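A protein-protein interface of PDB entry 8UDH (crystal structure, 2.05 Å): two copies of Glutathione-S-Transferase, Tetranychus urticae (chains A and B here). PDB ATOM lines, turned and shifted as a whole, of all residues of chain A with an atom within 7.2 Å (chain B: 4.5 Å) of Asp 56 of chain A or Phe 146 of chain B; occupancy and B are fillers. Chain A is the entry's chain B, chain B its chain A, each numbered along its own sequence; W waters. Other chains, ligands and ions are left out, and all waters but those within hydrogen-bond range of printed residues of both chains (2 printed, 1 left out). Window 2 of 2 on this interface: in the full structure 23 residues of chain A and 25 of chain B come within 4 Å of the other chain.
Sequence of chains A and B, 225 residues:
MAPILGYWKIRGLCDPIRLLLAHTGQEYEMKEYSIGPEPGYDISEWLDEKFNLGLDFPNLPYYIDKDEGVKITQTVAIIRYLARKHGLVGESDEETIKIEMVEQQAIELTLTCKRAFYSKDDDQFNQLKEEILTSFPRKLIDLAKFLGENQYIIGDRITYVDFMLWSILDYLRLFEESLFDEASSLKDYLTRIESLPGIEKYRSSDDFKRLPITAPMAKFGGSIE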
ATOM      1  N   LEU A  53      -6.789   9.787 -17.365  1.00  0.00           N
ATOM      2  CA  LEU A  53      -5.641  10.073 -16.515  1.00  0.00           C
ATOM      3  C   LEU A  53      -5.323  11.574 -16.476  1.00  0.00           C
ATOM      4  O   LEU A  53      -4.385  11.987 -15.802  1.00  0.00           O
ATOM      5  CB  LEU A  53      -4.459   9.258 -17.049  1.00  0.00           C
ATOM      6  CG  LEU A  53      -4.467   7.769 -16.688  1.00  0.00           C
ATOM      7  CD1 LEU A  53      -3.399   7.004 -17.473  1.00  0.00           C
ATOM      8  CD2 LEU A  53      -4.247   7.573 -15.191  1.00  0.00           C
ATOM      9  N   GLY A  54      -6.094  12.400 -17.195  1.00  0.00           N
ATOM     10  CA  GLY A  54      -5.859  13.838 -17.203  1.00  0.00           C
ATOM     11  C   GLY A  54      -4.701  14.250 -18.124  1.00  0.00           C
ATOM     12  O   GLY A  54      -4.231  15.367 -18.055  1.00  0.00           O
ATOM     13  N   LEU A  55      -4.282  13.359 -19.024  1.00  0.00           N
ATOM     14  CA  LEU A  55      -3.170  13.619 -19.910  1.00  0.00           C
ATOM     15  C   LEU A  55      -3.634  14.500 -21.064  1.00  0.00           C
ATOM     16  O   LEU A  55      -4.687  14.265 -21.675  1.00  0.00           O
ATOM     17  CB  LEU A  55      -2.637  12.288 -20.438  1.00  0.00           C
ATOM     18  CG  LEU A  55      -2.185  11.284 -19.372  1.00  0.00           C
ATOM     19  CD1 LEU A  55      -1.719  10.000 -20.043  1.00  0.00           C
ATOM     20  CD2 LEU A  55      -1.085  11.852 -18.497  1.00  0.00           C
ATOM     21  N   ASP A  56      -2.806  15.489 -21.416  1.00  0.00           N
ATOM     22  CA  ASP A  56      -3.115  16.348 -22.554  1.00  0.00           C
ATOM     23  C   ASP A  56      -3.019  15.581 -23.879  1.00  0.00           C
ATOM     24  O   ASP A  56      -3.810  15.827 -24.785  1.00  0.00           O
ATOM     25  CB  ASP A  56      -2.181  17.556 -22.569  1.00  0.00           C
ATOM     26  CG  ASP A  56      -2.423  18.465 -21.372  1.00  0.00           C
ATOM     27  OD1 ASP A  56      -3.495  19.067 -21.310  1.00  0.00           O
ATOM     28  OD2 ASP A  56      -1.531  18.541 -20.514  1.00  0.00           O
ATOM     29  N   PHE A  57      -2.009  14.704 -23.990  1.00  0.00           N
ATOM     30  CA  PHE A  57      -1.725  13.951 -25.202  1.00  0.00           C
ATOM     31  C   PHE A  57      -1.583  12.493 -24.799  1.00  0.00           C
ATOM     32  O   PHE A  57      -0.469  12.018 -24.604  1.00  0.00           O
ATOM     33  CB  PHE A  57      -0.455  14.418 -25.901  1.00  0.00           C
ATOM     34  CG  PHE A  57      -0.503  15.879 -26.232  1.00  0.00           C
ATOM     35  CD1 PHE A  57      -1.287  16.344 -27.278  1.00  0.00           C
ATOM     36  CD2 PHE A  57       0.183  16.787 -25.455  1.00  0.00           C
ATOM     37  CE1 PHE A  57      -1.388  17.698 -27.536  1.00  0.00           C
ATOM     38  CE2 PHE A  57       0.115  18.136 -25.744  1.00  0.00           C
ATOM     39  CZ  PHE A  57      -0.679  18.590 -26.775  1.00  0.00           C
ATOM     40  N   PRO A  58      -2.721  11.793 -24.573  1.00  0.00           N
ATOM     41  CA  PRO A  58      -2.707  10.477 -23.930  1.00  0.00           C
ATOM     42  C   PRO A  58      -1.813   9.521 -24.709  1.00  0.00           C
ATOM     43  O   PRO A  58      -1.936   9.410 -25.926  1.00  0.00           O
ATOM     44  CB  PRO A  58      -4.173  10.059 -24.002  1.00  0.00           C
ATOM     45  CG  PRO A  58      -4.900  11.379 -23.972  1.00  0.00           C
ATOM     46  CD  PRO A  58      -4.087  12.265 -24.870  1.00  0.00           C
ATOM     47  N   ASN A  59      -0.906   8.856 -23.994  1.00  0.00           N
ATOM     48  CA  ASN A  59       0.094   8.027 -24.642  1.00  0.00           C
ATOM     49  C   ASN A  59       0.903   7.301 -23.557  1.00  0.00           C
ATOM     50  O   ASN A  59       0.825   7.625 -22.376  1.00  0.00           O
ATOM     51  CB  ASN A  59       0.975   8.852 -25.587  1.00  0.00           C
ATOM     52  CG  ASN A  59       1.273   8.130 -26.885  1.00  0.00           C
ATOM     53  OD1 ASN A  59       1.344   6.907 -26.902  1.00  0.00           O
ATOM     54  ND2 ASN A  59       1.401   8.857 -27.987  1.00  0.00           N
ATOM     55  N   LYS A  71       1.981  16.143 -15.073  1.00  0.00           N
ATOM     56  CA  LYS A  71       1.488  15.037 -15.879  1.00  0.00           C
ATOM     57  C   LYS A  71       2.053  15.194 -17.277  1.00  0.00           C
ATOM     58  O   LYS A  71       1.725  16.160 -17.933  1.00  0.00           O
ATOM     59  CB  LYS A  71      -0.036  15.052 -15.967  1.00  0.00           C
ATOM     60  CG  LYS A  71      -0.727  14.942 -14.629  1.00  0.00           C
ATOM     61  CD  LYS A  71      -2.244  14.889 -14.779  1.00  0.00           C
ATOM     62  CE  LYS A  71      -2.930  14.545 -13.474  1.00  0.00           C
ATOM     63  NZ  LYS A  71      -4.268  13.960 -13.722  1.00  0.00           N
ATOM     64  N   ILE A  72       2.884  14.248 -17.704  1.00  0.00           N
ATOM     65  CA  ILE A  72       3.678  14.404 -18.915  1.00  0.00           C
ATOM     66  C   ILE A  72       3.524  13.135 -19.748  1.00  0.00           C
ATOM     67  O   ILE A  72       3.568  12.029 -19.221  1.00  0.00           O
ATOM     68  CB  ILE A  72       5.178  14.648 -18.588  1.00  0.00           C
ATOM     69  CG1 ILE A  72       5.392  15.616 -17.428  1.00  0.00           C
ATOM     70  CG2 ILE A  72       5.953  15.143 -19.801  1.00  0.00           C
ATOM     71  CD1 ILE A  72       6.865  15.809 -17.058  1.00  0.00           C
ATOM     72  N   THR A  73       3.366  13.306 -21.057  1.00  0.00           N
ATOM     73  CA  THR A  73       3.662  12.261 -22.016  1.00  0.00           C
ATOM     74  C   THR A  73       4.725  12.813 -22.956  1.00  0.00           C
ATOM     75  O   THR A  73       5.109  13.974 -22.829  1.00  0.00           O
ATOM     76  CB  THR A  73       2.399  11.828 -22.768  1.00  0.00           C
ATOM     77  OG1 THR A  73       1.879  12.927 -23.499  1.00  0.00           O
ATOM     78  CG2 THR A  73       1.361  11.254 -21.832  1.00  0.00           C
ATOM     79  N   GLN A  74       5.093  11.976 -23.921  1.00  0.00           N
ATOM     80  CA  GLN A  74       6.151  12.195 -24.879  1.00  0.00           C
ATOM     81  C   GLN A  74       7.482  11.851 -24.200  1.00  0.00           C
ATOM     82  O   GLN A  74       7.967  12.573 -23.331  1.00  0.00           O
ATOM     83  CB  GLN A  74       6.108  13.598 -25.486  1.00  0.00           C
ATOM     84  CG  GLN A  74       4.736  14.095 -25.927  1.00  0.00           C
ATOM     85  CD  GLN A  74       3.992  13.213 -26.922  1.00  0.00           C
ATOM     86  OE1 GLN A  74       4.473  12.950 -28.019  1.00  0.00           O
ATOM     87  NE2 GLN A  74       2.816  12.748 -26.552  1.00  0.00           N
ATOM     88  N   LYS B  98       5.219  22.060 -21.287  1.00  0.00           N
ATOM     89  CA  LYS B  98       4.174  22.217 -22.331  1.00  0.00           C
ATOM     90  C   LYS B  98       4.827  22.335 -23.713  1.00  0.00           C
ATOM     91  O   LYS B  98       4.391  21.624 -24.613  1.00  0.00           O
ATOM     92  CB  LYS B  98       3.303  23.429 -22.000  1.00  0.00           C
ATOM     93  CG  LYS B  98       2.399  23.281 -20.787  1.00  0.00           C
ATOM     94  CD  LYS B  98       1.613  24.534 -20.488  1.00  0.00           C
ATOM     95  CE  LYS B  98       0.670  24.366 -19.316  1.00  0.00           C
ATOM     96  NZ  LYS B  98       0.071  25.656 -18.902  1.00  0.00           N
ATOM     97  N   MET B 101       6.317  18.905 -24.787  1.00  0.00           N
ATOM     98  CA  MET B 101       5.265  17.926 -25.159  1.00  0.00           C
ATOM     99  C   MET B 101       4.764  18.235 -26.577  1.00  0.00           C
ATOM    100  O   MET B 101       4.671  17.306 -27.373  1.00  0.00           O
ATOM    101  CB  MET B 101       4.112  17.942 -24.152  1.00  0.00           C
ATOM    102  CG  MET B 101       4.378  17.085 -22.932  1.00  0.00           C
ATOM    103  SD  MET B 101       2.922  16.774 -21.908  1.00  0.00           S
ATOM    104  CE  MET B 101       2.264  18.430 -21.734  1.00  0.00           C
ATOM    105  N   VAL B 102       4.503  19.505 -26.875  1.00  0.00           N
ATOM    106  CA  VAL B 102       4.011  19.910 -28.225  1.00  0.00           C
ATOM    107  C   VAL B 102       5.120  19.732 -29.273  1.00  0.00           C
ATOM    108  O   VAL B 102       4.801  19.318 -30.376  1.00  0.00           O
ATOM    109  CB  VAL B 102       3.431  21.337 -28.207  1.00  0.00           C
ATOM    110  CG1 VAL B 102       2.922  21.757 -29.577  1.00  0.00           C
ATOM    111  CG2 VAL B 102       2.329  21.472 -27.170  1.00  0.00           C
ATOM    112  N   ASP B 142      -6.789  16.879 -30.024  1.00  0.00           N
ATOM    113  CA  ASP B 142      -5.962  16.975 -28.824  1.00  0.00           C
ATOM    114  C   ASP B 142      -5.145  18.259 -28.851  1.00  0.00           C
ATOM    115  O   ASP B 142      -5.066  18.933 -27.830  1.00  0.00           O
ATOM    116  CB  ASP B 142      -5.024  15.768 -28.667  1.00  0.00           C
ATOM    117  CG  ASP B 142      -5.765  14.486 -28.323  1.00  0.00           C
ATOM    118  OD1 ASP B 142      -6.888  14.567 -27.829  1.00  0.00           O
ATOM    119  OD2 ASP B 142      -5.248  13.427 -28.615  1.00  0.00           O
ATOM    120  N   LEU B 143      -4.569  18.617 -30.012  1.00  0.00           N
ATOM    121  CA  LEU B 143      -3.831  19.871 -30.102  1.00  0.00           C
ATOM    122  C   LEU B 143      -4.750  21.078 -29.897  1.00  0.00           C
ATOM    123  O   LEU B 143      -4.383  22.019 -29.177  1.00  0.00           O
ATOM    124  CB  LEU B 143      -3.068  19.933 -31.430  1.00  0.00           C
ATOM    125  CG  LEU B 143      -1.826  19.036 -31.466  1.00  0.00           C
ATOM    126  CD1 LEU B 143      -1.405  18.651 -32.887  1.00  0.00           C
ATOM    127  CD2 LEU B 143      -0.688  19.740 -30.727  1.00  0.00           C
ATOM    128  N   ALA B 144      -5.931  21.075 -30.523  1.00  0.00           N
ATOM    129  CA  ALA B 144      -6.890  22.165 -30.346  1.00  0.00           C
ATOM    130  C   ALA B 144      -7.313  22.312 -28.880  1.00  0.00           C
ATOM    131  O   ALA B 144      -7.450  23.426 -28.377  1.00  0.00           O
ATOM    132  CB  ALA B 144      -8.116  21.934 -31.218  1.00  0.00           C
ATOM    133  N   LYS B 145      -7.585  21.190 -28.206  1.00  0.00           N
ATOM    134  CA  LYS B 145      -7.971  21.246 -26.809  1.00  0.00           C
ATOM    135  C   LYS B 145      -6.844  21.862 -25.987  1.00  0.00           C
ATOM    136  O   LYS B 145      -7.076  22.669 -25.095  1.00  0.00           O
ATOM    137  CB  LYS B 145      -8.300  19.855 -26.263  1.00  0.00           C
ATOM    138  CG  LYS B 145      -9.613  19.279 -26.751  1.00  0.00           C
ATOM    139  CD  LYS B 145      -9.915  17.936 -26.141  1.00  0.00           C
ATOM    140  CE  LYS B 145     -10.115  18.035 -24.645  1.00  0.00           C
ATOM    141  NZ  LYS B 145     -10.361  16.704 -24.050  1.00  0.00           N
ATOM    142  N   PHE B 146      -5.613  21.458 -26.291  1.00  0.00           N
ATOM    143  CA  PHE B 146      -4.458  21.966 -25.565  1.00  0.00           C
ATOM    144  C   PHE B 146      -4.307  23.469 -25.766  1.00  0.00           C
ATOM    145  O   PHE B 146      -4.052  24.199 -24.822  1.00  0.00           O
ATOM    146  CB  PHE B 146      -3.199  21.230 -26.015  1.00  0.00           C
ATOM    147  CG  PHE B 146      -2.012  21.502 -25.147  1.00  0.00           C
ATOM    148  CD1 PHE B 146      -1.937  20.931 -23.894  1.00  0.00           C
ATOM    149  CD2 PHE B 146      -1.019  22.380 -25.544  1.00  0.00           C
ATOM    150  CE1 PHE B 146      -0.842  21.156 -23.081  1.00  0.00           C
ATOM    151  CE2 PHE B 146       0.060  22.631 -24.712  1.00  0.00           C
ATOM    152  CZ  PHE B 146       0.164  21.988 -23.506  1.00  0.00           C
ATOM    153  N   LEU B 147      -4.461  23.930 -27.004  1.00  0.00           N
ATOM    154  CA  LEU B 147      -4.369  25.344 -27.311  1.00  0.00           C
ATOM    155  C   LEU B 147      -5.494  26.107 -26.612  1.00  0.00           C
ATOM    156  O   LEU B 147      -5.274  27.201 -26.109  1.00  0.00           O
ATOM    157  CB  LEU B 147      -4.433  25.523 -28.823  1.00  0.00           C
ATOM    158  CG  LEU B 147      -4.360  26.958 -29.321  1.00  0.00           C
ATOM    159  CD1 LEU B 147      -2.933  27.528 -29.102  1.00  0.00           C
ATOM    160  CD2 LEU B 147      -4.780  27.032 -30.772  1.00  0.00           C
ATOM    161  N   GLY B 148      -6.697  25.519 -26.579  1.00  0.00           N
ATOM    162  CA  GLY B 148      -7.853  26.174 -25.993  1.00  0.00           C
ATOM    163  C   GLY B 148      -8.098  27.542 -26.623  1.00  0.00           C
ATOM    164  O   GLY B 148      -8.076  27.689 -27.847  1.00  0.00           O
ATOM    165  N   ILE B 153       0.842  28.270 -28.080  1.00  0.00           N
ATOM    166  CA  ILE B 153       0.910  27.097 -27.209  1.00  0.00           C
ATOM    167  C   ILE B 153       1.018  27.414 -25.718  1.00  0.00           C
ATOM    168  O   ILE B 153       0.418  26.712 -24.914  1.00  0.00           O
ATOM    169  CB  ILE B 153       2.072  26.183 -27.684  1.00  0.00           C
ATOM    170  CG1 ILE B 153       1.689  25.519 -29.017  1.00  0.00           C
ATOM    171  CG2 ILE B 153       2.529  25.175 -26.599  1.00  0.00           C
ATOM    172  CD1 ILE B 153       0.437  24.664 -28.953  1.00  0.00           C
HETATM  173  O   HOH W   1      -5.227  17.972 -25.345  1.00  0.00           O
HETATM  174  O   HOH W   2       0.129  14.428 -21.962  1.00  0.00           O
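CE of Met 101 of chain B touches OD2 of Asp 56 of chain A, 3.99 Å away.
Asp 56 of chain A touches Phe 146 of chain B.
CE1 of Phe 57 of chain A touches O of Asp 142 of chain B, 3.9 Å away.
Phe 57 of chain A touches Leu 143 of chain B (CE1 to CD2, 3.9 Å).
Phe 57 of chain A touches Phe 146 of chain B (CZ to CG, 3.6 Å).
Ile 72 of chain A touches Met 101 of chain B (CA to SD, 3.9 Å).
Gln 74 of chain A touches Met 101 of chain B (CG to O, 3.5 Å).
Printed residues of chain A that touch a printed residue of chain B: Asp 56, Phe 57, Ile 72, Thr 73 and Gln 74.
Hydrophobic or aromatic side chains of chain A that line the printed part of chain B: Phe 57.
Along chain B the printed residues that touch a printed residue of chain A span positions 101 to 146.
Water W1 lies within hydrogen-bond range of O of Asp 56 of chain A (2.6 Å) and O of Asp 142 of chain B (2.7 Å).
Water W2 lies within hydrogen-bond range of OG1 of Thr 73 of chain A (2.8 Å), N of Phe 57 of chain A (3.0 Å), N of Asp 56 of chain A (3.2 Å) and SD of Met 101 of chain B (3.6 Å).
Printed residues of chain B within 4 Å of Asp 56 of chain A: Met 101 and Phe 146.
Of the printed residues of chain A, Met 101 of chain B touches Asp 56, Ile 72, Thr 73 and Gln 74.
Printed residues of chain A within 4 Å of Asp 142 of chain B: Phe 57 (3.9 Å).
Of the printed residues of chain A, Leu 143 of chain B touches Phe 57.
Of the printed residues of chain A, Phe 146 of chain B touches Asp 56 and Phe 57.
The nearest printed residue of chain B that does not touch Asp 56 of chain A is Asp 142 of chain B (4.1 Å).
The nearest printed residue of chain A that does not touch Phe 146 of chain B is Leu 55 of chain A (7.2 Å).
The nearest printed residue of chain B that does not touch Phe 57 of chain A is Val 102 of chain B (4.2 Å).
N of Thr 73 of chain A lies within hydrogen-bond range of SD of Met 101 of chain B (3.6 Å).
OG1 of Thr 73 of chain A sits at hydrogen-bond distance from NE2 of Gln 74 of chain A, at 3.2 Å.
O of Phe 57 of chain A lies within hydrogen-bond range of OG1 of Thr 73 of chain A (2.7 Å).
No position is printed for both chains.
Of the 8 pairs that touch across the chains among the printed residues, none has its exchanged pair printed and touching as well.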
